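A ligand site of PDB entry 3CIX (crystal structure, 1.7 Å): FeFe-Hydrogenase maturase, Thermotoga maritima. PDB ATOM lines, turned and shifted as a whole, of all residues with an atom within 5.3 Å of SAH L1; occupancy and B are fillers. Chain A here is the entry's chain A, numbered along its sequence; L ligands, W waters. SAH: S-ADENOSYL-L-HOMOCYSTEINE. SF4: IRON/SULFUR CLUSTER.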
ATOM      1  N   CYS A  63       7.681  -9.749  18.583  1.00  0.00           N
ATOM      2  CA  CYS A  63       8.029  -8.923  17.422  1.00  0.00           C
ATOM      3  C   CYS A  63       9.473  -8.484  17.449  1.00  0.00           C
ATOM      4  O   CYS A  63      10.004  -8.109  18.498  1.00  0.00           O
ATOM      5  CB  CYS A  63       7.126  -7.706  17.280  1.00  0.00           C
ATOM      6  SG  CYS A  63       7.275  -6.939  15.632  1.00  0.00           S
ATOM      7  N   TYR A  69       4.613   3.472  17.642  1.00  0.00           N
ATOM      8  CA  TYR A  69       3.209   3.504  18.101  1.00  0.00           C
ATOM      9  C   TYR A  69       2.721   2.204  18.769  1.00  0.00           C
ATOM     10  O   TYR A  69       1.690   2.200  19.460  1.00  0.00           O
ATOM     11  CB  TYR A  69       2.293   3.813  16.913  1.00  0.00           C
ATOM     12  CG  TYR A  69       2.603   3.034  15.682  1.00  0.00           C
ATOM     13  CD1 TYR A  69       2.167   1.705  15.531  1.00  0.00           C
ATOM     14  CD2 TYR A  69       3.363   3.601  14.640  1.00  0.00           C
ATOM     15  CE1 TYR A  69       2.472   0.999  14.376  1.00  0.00           C
ATOM     16  CE2 TYR A  69       3.668   2.883  13.503  1.00  0.00           C
ATOM     17  CZ  TYR A  69       3.198   1.589  13.376  1.00  0.00           C
ATOM     18  OH  TYR A  69       3.513   0.883  12.244  1.00  0.00           O
ATOM     19  N   CYS A  70       3.447   1.111  18.570  1.00  0.00           N
ATOM     20  CA  CYS A  70       2.907  -0.224  18.820  1.00  0.00           C
ATOM     21  C   CYS A  70       3.324  -0.802  20.165  1.00  0.00           C
ATOM     22  O   CYS A  70       4.525  -0.804  20.506  1.00  0.00           O
ATOM     23  CB  CYS A  70       3.352  -1.171  17.718  1.00  0.00           C
ATOM     24  SG  CYS A  70       2.568  -2.788  17.861  1.00  0.00           S
ATOM     25  N   GLY A  71       2.351  -1.307  20.922  1.00  0.00           N
ATOM     26  CA  GLY A  71       2.599  -1.950  22.191  1.00  0.00           C
ATOM     27  C   GLY A  71       3.398  -3.246  22.123  1.00  0.00           C
ATOM     28  O   GLY A  71       3.989  -3.656  23.121  1.00  0.00           O
ATOM     29  N   GLN A 107      -2.833 -13.411  12.497  1.00  0.00           N
ATOM     30  CA  GLN A 107      -2.083 -12.175  12.733  1.00  0.00           C
ATOM     31  C   GLN A 107      -1.088 -12.364  13.857  1.00  0.00           C
ATOM     32  O   GLN A 107      -1.381 -13.049  14.836  1.00  0.00           O
ATOM     33  CB  GLN A 107      -3.005 -10.984  13.044  1.00  0.00           C
ATOM     34  CG  GLN A 107      -2.288  -9.652  13.049  1.00  0.00           C
ATOM     35  CD  GLN A 107      -3.206  -8.455  13.352  1.00  0.00           C
ATOM     36  OE1 GLN A 107      -3.538  -8.182  14.506  1.00  0.00           O
ATOM     37  NE2 GLN A 107      -3.628  -7.784  12.309  1.00  0.00           N
ATOM     38  N   SER A 108       0.081 -11.738  13.699  1.00  0.00           N
ATOM     39  CA  SER A 108       1.092 -11.785  14.750  1.00  0.00           C
ATOM     40  C   SER A 108       2.000 -10.582  14.687  1.00  0.00           C
ATOM     41  O   SER A 108       2.026  -9.816  13.699  1.00  0.00           O
ATOM     42  CB  SER A 108       1.910 -13.076  14.610  1.00  0.00           C
ATOM     43  OG  SER A 108       2.583 -13.092  13.353  1.00  0.00           O
ATOM     44  N   GLY A 109       2.827 -10.437  15.719  1.00  0.00           N
ATOM     45  CA  GLY A 109       4.013  -9.591  15.575  1.00  0.00           C
ATOM     46  C   GLY A 109       4.928 -10.249  14.550  1.00  0.00           C
ATOM     47  O   GLY A 109       4.687 -11.376  14.141  1.00  0.00           O
ATOM     48  N   GLU A 110       5.952  -9.541  14.109  1.00  0.00           N
ATOM     49  CA  GLU A 110       6.956 -10.138  13.239  1.00  0.00           C
ATOM     50  C   GLU A 110       7.848 -11.066  14.057  1.00  0.00           C
ATOM     51  O   GLU A 110       8.958 -10.681  14.520  1.00  0.00           O
ATOM     52  CB  GLU A 110       7.771  -9.069  12.498  1.00  0.00           C
ATOM     53  CG  GLU A 110       6.953  -8.297  11.412  1.00  0.00           C
ATOM     54  CD  GLU A 110       7.836  -7.502  10.442  1.00  0.00           C
ATOM     55  OE1 GLU A 110       9.096  -7.646  10.503  1.00  0.00           O
ATOM     56  OE2 GLU A 110       7.270  -6.727   9.621  1.00  0.00           O
ATOM     57  N   SER A 136      -1.634 -11.806   8.163  1.00  0.00           N
ATOM     58  CA  SER A 136      -1.250 -10.453   8.568  1.00  0.00           C
ATOM     59  C   SER A 136      -0.031 -10.604   9.467  1.00  0.00           C
ATOM     60  O   SER A 136      -0.111 -10.435  10.673  1.00  0.00           O
ATOM     61  CB  SER A 136      -2.419  -9.774   9.274  1.00  0.00           C
ATOM     62  OG  SER A 136      -2.156  -8.426   9.628  1.00  0.00           O
ATOM     63  N   LEU A 137       1.117 -10.894   8.841  1.00  0.00           N
ATOM     64  CA  LEU A 137       2.363 -11.209   9.552  1.00  0.00           C
ATOM     65  C   LEU A 137       3.482 -10.180   9.366  1.00  0.00           C
ATOM     66  O   LEU A 137       4.591 -10.406   9.863  1.00  0.00           O
ATOM     67  CB  LEU A 137       2.882 -12.573   9.101  1.00  0.00           C
ATOM     68  CG  LEU A 137       1.876 -13.721   9.017  1.00  0.00           C
ATOM     69  CD1 LEU A 137       2.481 -15.025   8.482  1.00  0.00           C
ATOM     70  CD2 LEU A 137       1.126 -13.965  10.381  1.00  0.00           C
ATOM     71  N   GLY A 138       3.217  -9.063   8.681  1.00  0.00           N
ATOM     72  CA  GLY A 138       4.246  -8.056   8.448  1.00  0.00           C
ATOM     73  C   GLY A 138       5.091  -8.266   7.171  1.00  0.00           C
ATOM     74  O   GLY A 138       4.643  -8.851   6.195  1.00  0.00           O
ATOM     75  N   LEU A 157      -3.132  -8.955   4.666  1.00  0.00           N
ATOM     76  CA  LEU A 157      -3.374  -7.613   5.155  1.00  0.00           C
ATOM     77  C   LEU A 157      -2.043  -7.006   5.599  1.00  0.00           C
ATOM     78  O   LEU A 157      -1.384  -7.532   6.506  1.00  0.00           O
ATOM     79  CB  LEU A 157      -4.323  -7.607   6.349  1.00  0.00           C
ATOM     80  CG  LEU A 157      -5.787  -8.019   6.199  1.00  0.00           C
ATOM     81  CD1 LEU A 157      -6.330  -8.423   7.566  1.00  0.00           C
ATOM     82  CD2 LEU A 157      -6.658  -6.888   5.589  1.00  0.00           C
ATOM     83  N   LEU A 158      -1.681  -5.908   4.967  1.00  0.00           N
ATOM     84  CA  LEU A 158      -0.418  -5.171   5.262  1.00  0.00           C
ATOM     85  C   LEU A 158      -0.671  -3.671   5.144  1.00  0.00           C
ATOM     86  O   LEU A 158      -0.464  -3.048   4.085  1.00  0.00           O
ATOM     87  CB  LEU A 158       0.712  -5.657   4.363  1.00  0.00           C
ATOM     88  CG  LEU A 158       2.126  -5.194   4.746  1.00  0.00           C
ATOM     89  CD1 LEU A 158       2.655  -5.968   5.974  1.00  0.00           C
ATOM     90  CD2 LEU A 158       3.089  -5.394   3.567  1.00  0.00           C
ATOM     91  N   ARG A 159      -1.187  -3.098   6.227  1.00  0.00           N
ATOM     92  CA  ARG A 159      -1.554  -1.696   6.218  1.00  0.00           C
ATOM     93  C   ARG A 159      -0.322  -0.893   5.828  1.00  0.00           C
ATOM     94  O   ARG A 159       0.769  -1.167   6.331  1.00  0.00           O
ATOM     95  CB  ARG A 159      -2.006  -1.301   7.595  1.00  0.00           C
ATOM     96  CG  ARG A 159      -3.323  -1.888   7.975  1.00  0.00           C
ATOM     97  CD  ARG A 159      -3.866  -1.071   9.093  1.00  0.00           C
ATOM     98  NE  ARG A 159      -5.000  -1.677   9.717  1.00  0.00           N
ATOM     99  CZ  ARG A 159      -5.589  -1.188  10.798  1.00  0.00           C
ATOM    100  NH1 ARG A 159      -5.123  -0.075  11.337  1.00  0.00           N
ATOM    101  NH2 ARG A 159      -6.646  -1.814  11.305  1.00  0.00           N
ATOM    102  N   GLU A 161       0.138   2.145   6.590  1.00  0.00           N
ATOM    103  CA  GLU A 161       0.339   2.929   7.836  1.00  0.00           C
ATOM    104  C   GLU A 161       0.297   4.444   7.614  1.00  0.00           C
ATOM    105  O   GLU A 161      -0.516   5.143   8.222  1.00  0.00           O
ATOM    106  CB  GLU A 161       1.617   2.549   8.585  1.00  0.00           C
ATOM    107  CG  GLU A 161       1.830   1.017   8.750  1.00  0.00           C
ATOM    108  CD  GLU A 161       0.770   0.323   9.596  1.00  0.00           C
ATOM    109  OE1 GLU A 161      -0.278   0.912   9.959  1.00  0.00           O
ATOM    110  OE2 GLU A 161       1.017  -0.879   9.899  1.00  0.00           O
ATOM    111  N   ARG A 172       8.655   4.004  11.994  1.00  0.00           N
ATOM    112  CA  ARG A 172       8.940   2.601  11.745  1.00  0.00           C
ATOM    113  C   ARG A 172      10.440   2.491  11.411  1.00  0.00           C
ATOM    114  O   ARG A 172      10.815   2.298  10.252  1.00  0.00           O
ATOM    115  CB  ARG A 172       8.025   2.074  10.645  1.00  0.00           C
ATOM    116  CG  ARG A 172       6.540   2.409  10.877  1.00  0.00           C
ATOM    117  CD  ARG A 172       5.592   1.630   9.947  1.00  0.00           C
ATOM    118  NE  ARG A 172       5.677   0.204  10.245  1.00  0.00           N
ATOM    119  CZ  ARG A 172       6.151  -0.720   9.417  1.00  0.00           C
ATOM    120  NH1 ARG A 172       6.501  -0.402   8.177  1.00  0.00           N
ATOM    121  NH2 ARG A 172       6.284  -1.974   9.853  1.00  0.00           N
ATOM    122  N   ARG A 180       7.638  -1.062   2.392  1.00  0.00           N
ATOM    123  CA  ARG A 180       6.235  -1.438   2.624  1.00  0.00           C
ATOM    124  C   ARG A 180       5.490  -1.529   1.294  1.00  0.00           C
ATOM    125  O   ARG A 180       4.769  -2.500   1.014  1.00  0.00           O
ATOM    126  CB  ARG A 180       5.572  -0.406   3.532  1.00  0.00           C
ATOM    127  CG  ARG A 180       4.275  -0.853   4.195  1.00  0.00           C
ATOM    128  CD  ARG A 180       4.567  -1.738   5.381  1.00  0.00           C
ATOM    129  NE  ARG A 180       3.398  -2.023   6.180  1.00  0.00           N
ATOM    130  CZ  ARG A 180       3.413  -2.845   7.233  1.00  0.00           C
ATOM    131  NH1 ARG A 180       4.522  -3.496   7.562  1.00  0.00           N
ATOM    132  NH2 ARG A 180       2.301  -3.074   7.940  1.00  0.00           N
ATOM    133  N   MET A 199      -3.239   4.507   9.622  1.00  0.00           N
ATOM    134  CA  MET A 199      -3.760   5.041  10.872  1.00  0.00           C
ATOM    135  C   MET A 199      -4.031   6.534  10.664  1.00  0.00           C
ATOM    136  O   MET A 199      -3.411   7.186   9.816  1.00  0.00           O
ATOM    137  CB  MET A 199      -2.798   4.831  12.030  1.00  0.00           C
ATOM    138  CG  MET A 199      -2.724   3.377  12.547  1.00  0.00           C
ATOM    139  SD  MET A 199      -1.403   3.133  13.781  1.00  0.00           S
ATOM    140  CE  MET A 199       0.018   3.049  12.742  1.00  0.00           C
ATOM    141  N   PRO A 229      -7.996   4.753  14.003  1.00  0.00           N
ATOM    142  CA  PRO A 229      -7.369   5.873  14.664  1.00  0.00           C
ATOM    143  C   PRO A 229      -6.125   5.401  15.383  1.00  0.00           C
ATOM    144  O   PRO A 229      -6.101   4.292  15.923  1.00  0.00           O
ATOM    145  CB  PRO A 229      -8.432   6.312  15.682  1.00  0.00           C
ATOM    146  CG  PRO A 229      -9.079   5.038  16.067  1.00  0.00           C
ATOM    147  CD  PRO A 229      -9.130   4.233  14.778  1.00  0.00           C
ATOM    148  N   PHE A 230      -5.105   6.265  15.431  1.00  0.00           N
ATOM    149  CA  PHE A 230      -4.014   6.061  16.365  1.00  0.00           C
ATOM    150  C   PHE A 230      -4.471   6.129  17.834  1.00  0.00           C
ATOM    151  O   PHE A 230      -5.141   7.085  18.243  1.00  0.00           O
ATOM    152  CB  PHE A 230      -2.938   7.109  16.093  1.00  0.00           C
ATOM    153  CG  PHE A 230      -1.906   7.206  17.183  1.00  0.00           C
ATOM    154  CD1 PHE A 230      -1.078   6.127  17.473  1.00  0.00           C
ATOM    155  CD2 PHE A 230      -1.745   8.387  17.899  1.00  0.00           C
ATOM    156  CE1 PHE A 230      -0.129   6.213  18.484  1.00  0.00           C
ATOM    157  CE2 PHE A 230      -0.793   8.455  18.883  1.00  0.00           C
ATOM    158  CZ  PHE A 230       0.000   7.366  19.172  1.00  0.00           C
ATOM    159  N   ILE A 231      -4.118   5.111  18.617  1.00  0.00           N
ATOM    160  CA  ILE A 231      -4.415   5.028  20.053  1.00  0.00           C
ATOM    161  C   ILE A 231      -3.084   4.916  20.820  1.00  0.00           C
ATOM    162  O   ILE A 231      -2.413   3.885  20.744  1.00  0.00           O
ATOM    163  CB  ILE A 231      -5.379   3.854  20.417  1.00  0.00           C
ATOM    164  CG1 ILE A 231      -6.711   3.965  19.632  1.00  0.00           C
ATOM    165  CG2 ILE A 231      -5.647   3.840  21.931  1.00  0.00           C
ATOM    166  CD1 ILE A 231      -7.634   2.764  19.761  1.00  0.00           C
ATOM    167  N   PRO A 232      -2.681   5.970  21.563  1.00  0.00           N
ATOM    168  CA  PRO A 232      -1.367   5.900  22.223  1.00  0.00           C
ATOM    169  C   PRO A 232      -1.279   4.799  23.298  1.00  0.00           C
ATOM    170  O   PRO A 232      -2.240   4.534  24.038  1.00  0.00           O
ATOM    171  CB  PRO A 232      -1.191   7.295  22.815  1.00  0.00           C
ATOM    172  CG  PRO A 232      -2.586   7.812  22.970  1.00  0.00           C
ATOM    173  CD  PRO A 232      -3.353   7.261  21.810  1.00  0.00           C
ATOM    174  N   HIS A 233      -0.120   4.135  23.337  1.00  0.00           N
ATOM    175  CA  HIS A 233       0.077   3.012  24.238  1.00  0.00           C
ATOM    176  C   HIS A 233       1.073   3.497  25.293  1.00  0.00           C
ATOM    177  O   HIS A 233       2.097   4.058  24.958  1.00  0.00           O
ATOM    178  CB  HIS A 233       0.646   1.824  23.458  1.00  0.00           C
ATOM    179  CG  HIS A 233       0.687   0.559  24.253  1.00  0.00           C
ATOM    180  ND1 HIS A 233       1.475   0.415  25.360  1.00  0.00           N
ATOM    181  CD2 HIS A 233       0.033  -0.624  24.096  1.00  0.00           C
ATOM    182  CE1 HIS A 233       1.303  -0.789  25.870  1.00  0.00           C
ATOM    183  NE2 HIS A 233       0.430  -1.444  25.125  1.00  0.00           N
ATOM    184  N   ALA A 270     -10.075  -0.903  16.505  1.00  0.00           N
ATOM    185  CA  ALA A 270      -9.645   0.386  17.044  1.00  0.00           C
ATOM    186  C   ALA A 270     -10.788   1.408  17.037  1.00  0.00           C
ATOM    187  O   ALA A 270     -10.942   2.206  17.999  1.00  0.00           O
ATOM    188  CB  ALA A 270      -8.413   0.939  16.286  1.00  0.00           C
ATOM    189  N   TYR A 303      -2.217  -9.396  23.750  1.00  0.00           N
ATOM    190  CA  TYR A 303      -2.020  -8.855  22.420  1.00  0.00           C
ATOM    191  C   TYR A 303      -2.479  -7.399  22.415  1.00  0.00           C
ATOM    192  O   TYR A 303      -3.569  -7.090  21.973  1.00  0.00           O
ATOM    193  CB  TYR A 303      -2.737  -9.722  21.380  1.00  0.00           C
ATOM    194  CG  TYR A 303      -2.285  -9.447  19.975  1.00  0.00           C
ATOM    195  CD1 TYR A 303      -1.130 -10.050  19.445  1.00  0.00           C
ATOM    196  CD2 TYR A 303      -2.988  -8.562  19.164  1.00  0.00           C
ATOM    197  CE1 TYR A 303      -0.748  -9.850  18.135  1.00  0.00           C
ATOM    198  CE2 TYR A 303      -2.587  -8.337  17.845  1.00  0.00           C
ATOM    199  CZ  TYR A 303      -1.454  -8.970  17.348  1.00  0.00           C
ATOM    200  OH  TYR A 303      -1.039  -8.774  16.042  1.00  0.00           O
ATOM    201  N   LEU A 305      -1.684  -4.133  21.065  1.00  0.00           N
ATOM    202  CA  LEU A 305      -1.126  -3.156  20.097  1.00  0.00           C
ATOM    203  C   LEU A 305      -1.362  -1.764  20.662  1.00  0.00           C
ATOM    204  O   LEU A 305      -0.501  -0.893  20.586  1.00  0.00           O
ATOM    205  CB  LEU A 305      -1.783  -3.269  18.713  1.00  0.00           C
ATOM    206  CG  LEU A 305      -1.808  -4.635  18.021  1.00  0.00           C
ATOM    207  CD1 LEU A 305      -2.779  -4.622  16.817  1.00  0.00           C
ATOM    208  CD2 LEU A 305      -0.419  -5.028  17.588  1.00  0.00           C
ATOM    209  N   TYR A 306      -2.574  -1.589  21.206  1.00  0.00           N
ATOM    210  CA  TYR A 306      -3.005  -0.391  21.890  1.00  0.00           C
ATOM    211  C   TYR A 306      -3.832  -0.833  23.103  1.00  0.00           C
ATOM    212  O   TYR A 306      -4.376  -1.949  23.103  1.00  0.00           O
ATOM    213  CB  TYR A 306      -3.845   0.496  20.936  1.00  0.00           C
ATOM    214  CG  TYR A 306      -4.907  -0.277  20.145  1.00  0.00           C
ATOM    215  CD1 TYR A 306      -6.138  -0.584  20.708  1.00  0.00           C
ATOM    216  CD2 TYR A 306      -4.662  -0.668  18.848  1.00  0.00           C
ATOM    217  CE1 TYR A 306      -7.098  -1.310  20.008  1.00  0.00           C
ATOM    218  CE2 TYR A 306      -5.609  -1.398  18.123  1.00  0.00           C
ATOM    219  CZ  TYR A 306      -6.820  -1.705  18.713  1.00  0.00           C
ATOM    220  OH  TYR A 306      -7.744  -2.417  17.990  1.00  0.00           O
HETATM  221  N   SAH L   1       3.062  -7.060  12.700  1.00  0.00           N
HETATM  222  CA  SAH L   1       2.085  -6.940  11.557  1.00  0.00           C
HETATM  223  CB  SAH L   1       0.646  -7.292  11.994  1.00  0.00           C
HETATM  224  CG  SAH L   1       0.194  -6.791  13.362  1.00  0.00           C
HETATM  225  SD  SAH L   1       0.104  -5.003  13.617  1.00  0.00           S
HETATM  226  C   SAH L   1       2.160  -5.585  10.869  1.00  0.00           C
HETATM  227  O   SAH L   1       2.781  -4.665  11.379  1.00  0.00           O
HETATM  228  OXT SAH L   1       1.622  -5.414   9.752  1.00  0.00           O
HETATM  229  C5' SAH L   1      -1.615  -4.662  13.028  1.00  0.00           C
HETATM  230  C4' SAH L   1      -2.017  -3.177  12.805  1.00  0.00           C
HETATM  231  O4' SAH L   1      -2.376  -2.535  14.047  1.00  0.00           O
HETATM  232  C3' SAH L   1      -0.965  -2.250  12.220  1.00  0.00           C
HETATM  233  O3' SAH L   1      -0.880  -2.332  10.814  1.00  0.00           O
HETATM  234  C2' SAH L   1      -1.325  -0.867  12.759  1.00  0.00           C
HETATM  235  O2' SAH L   1      -1.955  -0.054  11.812  1.00  0.00           O
HETATM  236  C1' SAH L   1      -2.275  -1.155  13.943  1.00  0.00           C
HETATM  237  N9  SAH L   1      -1.724  -0.551  15.162  1.00  0.00           N
HETATM  238  C8  SAH L   1      -0.537  -0.823  15.801  1.00  0.00           C
HETATM  239  N7  SAH L   1      -0.416  -0.019  16.868  1.00  0.00           N
HETATM  240  C5  SAH L   1      -1.509   0.809  16.913  1.00  0.00           C
HETATM  241  C6  SAH L   1      -1.912   1.800  17.786  1.00  0.00           C
HETATM  242  N6  SAH L   1      -1.172   2.229  18.837  1.00  0.00           N
HETATM  243  N1  SAH L   1      -3.131   2.408  17.542  1.00  0.00           N
HETATM  244  C2  SAH L   1      -3.941   2.038  16.499  1.00  0.00           C
HETATM  245  N3  SAH L   1      -3.552   1.051  15.650  1.00  0.00           N
HETATM  246  C4  SAH L   1      -2.357   0.437  15.874  1.00  0.00           C
HETATM  247 FE1  SF4 L   2       5.399  -2.882  14.158  1.00  0.00          FE
HETATM  248 FE2  SF4 L   2       3.466  -4.943  13.556  1.00  0.00          FE
HETATM  249 FE3  SF4 L   2       5.720  -5.333  15.322  1.00  0.00          FE
HETATM  250 FE4  SF4 L   2       3.691  -3.729  16.098  1.00  0.00          FE
HETATM  251  S1  SF4 L   2       3.510  -5.972  15.683  1.00  0.00           S
HETATM  252  S2  SF4 L   2       5.977  -3.326  16.343  1.00  0.00           S
HETATM  253  S3  SF4 L   2       3.067  -2.711  14.097  1.00  0.00           S
HETATM  254  S4  SF4 L   2       5.772  -4.849  13.068  1.00  0.00           S
HETATM  255  O   HOH W   1      -4.942  -3.684  14.250  1.00  0.00           O
HETATM  256  O   HOH W   2      -0.924  -4.341   8.996  1.00  0.00           O
HETATM  257  O   HOH W   3       5.229  -5.063   9.822  1.00  0.00           O
HETATM  258  O   HOH W   4      -5.881   0.895  13.915  1.00  0.00           O
HETATM  259  O   HOH W   5       0.587  -7.643   8.371  1.00  0.00           O
HETATM  260  O   HOH W   6       3.344  -1.641  11.012  1.00  0.00           O
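An oxygen (O3') of SAH L1 lies within hydrogen-bond range of the side-chain carboxylate of Glu 161, 2.6 Å away. N of Ile 231 sits at hydrogen-bond distance from N1 of SAH L1 (3.1 Å). The backbone carbonyl oxygen of Ile 231 lies within hydrogen-bond range of a nitrogen (N6) of SAH L1 (2.8 Å). N6 of SAH L1 is in hydrogen-bond range of O of Tyr 69. OXT of SAH L1 is in salt-bridge range of NH2 of Arg 180 (3.0 Å). O of Ser 108 sits close to N of SAH L1, 3.1 Å away. NH1 of Arg 159 sits at hydrogen-bond distance from O2' of SAH L1 (3.2 Å). SD of Met 199 lies close to O2' of SAH L1, at 3.8 Å. SG of Cys 70 binds FE4 of SF4 L2 (2.3 Å). An iron atom (FE3) of SF4 L2 is bound by the side-chain sulfur (SG) of Cys 63.
An oxygen (O) of SAH L1 is bound to an iron atom (FE2) of SF4 L2, 2.3 Å away.
OE2 of Glu 161 is in salt-bridge range of NH2 of Arg 180, at 3.2 Å. The backbone carbonyl oxygen (O) of Glu 161 lies within hydrogen-bond range of the backbone NH (N) of Met 199, at 3.1 Å. The side-chain hydroxyl of Tyr 69 sits at hydrogen-bond distance from the guanidinium group of Arg 172. The backbone carbonyl oxygen of Arg 159 is in hydrogen-bond range of the guanidinium group of Arg 180 (2.8 Å). The backbone carbonyl oxygen (O) of Leu 305 lies within hydrogen-bond range of the backbone NH (N) of Gly 71 (2.9 Å). The side-chain amide nitrogen of Gln 107 lies within hydrogen-bond range of the side-chain hydroxyl of Ser 136, 3.1 Å away. The backbone carbonyl oxygen (O) of Leu 157 lies within hydrogen-bond range of the side-chain hydroxyl (OG) of Ser 136 (3.3 Å). OH of Tyr 303 is in hydrogen-bond range of OE1 of Gln 107 (3.0 Å).
CA of Cys 70 touches N7 of SAH L1, at 3.9 Å. Gln 107 touches SAH L1 (NE2 to C5', 3.8 Å). CA of Gly 109 touches N of SAH L1 (3.9 Å). O of Ser 136 touches CB of SAH L1, 3.5 Å away. Gly 138 touches SAH L1 (N to CA, 3.7 Å). Leu 158 touches SAH L1 (CD1 to OXT, 3.96 Å). Pro 229 touches SAH L1 (O to C2, 3.2 Å). Phe 230 touches SAH L1. OH of Tyr 303 touches CG of SAH L1, at 3.6 Å. CD1 of Leu 305 touches O4' of SAH L1 (3.5 Å). CD2 of Tyr 306 touches C2 of SAH L1, 3.7 Å away. Hydrophobic or aromatic side chains within 4 Å of SAH L1: Tyr 69, Leu 158, Met 199, Ile 231, Leu 305 and Tyr 306. Within 4 Å of SAH L1: Tyr 69, Cys 70, Gln 107, Ser 108, Gly 109, Ser 136, Gly 138, Leu 158, Arg 159, Glu 161, Arg 180, Met 199, Pro 229, Phe 230, Ile 231, Tyr 303, Leu 305 and Tyr 306. The nearest printed residue that does not touch SAH L1 is Glu 110 (4.1 Å).
Water W2 lies within hydrogen-bond range of O3' of SAH L1 (2.7 Å) and N of Arg 159 (3.0 Å). Water W5 lies within hydrogen-bond range of O of Leu 157 (2.7 Å), OXT of SAH L1 (2.8 Å), N of Gly 138 (3.0 Å), OG of Ser 136 (3.1 Å) and N of Leu 137 (3.3 Å). Water W4 bridges the guanidinium group (NH1) of Arg 159 and a nitrogen (N3) of SAH L1. Water W3 lies within hydrogen-bond range of the side-chain carboxylate of Glu 110 (2.6 Å), the guanidinium group of Arg 180 (2.8 Å), the guanidinium group of Arg 172 (3.3 Å) and a sulfur (S4) of SF4 L2 (3.3 Å). Water W6 lies within hydrogen-bond range of the side-chain carboxylate of Glu 161 (2.7 Å), the side-chain hydroxyl of Tyr 69 (2.8 Å), the guanidinium group of Arg 172 (3.1 Å) and a sulfur (S3) of SF4 L2 (3.3 Å).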
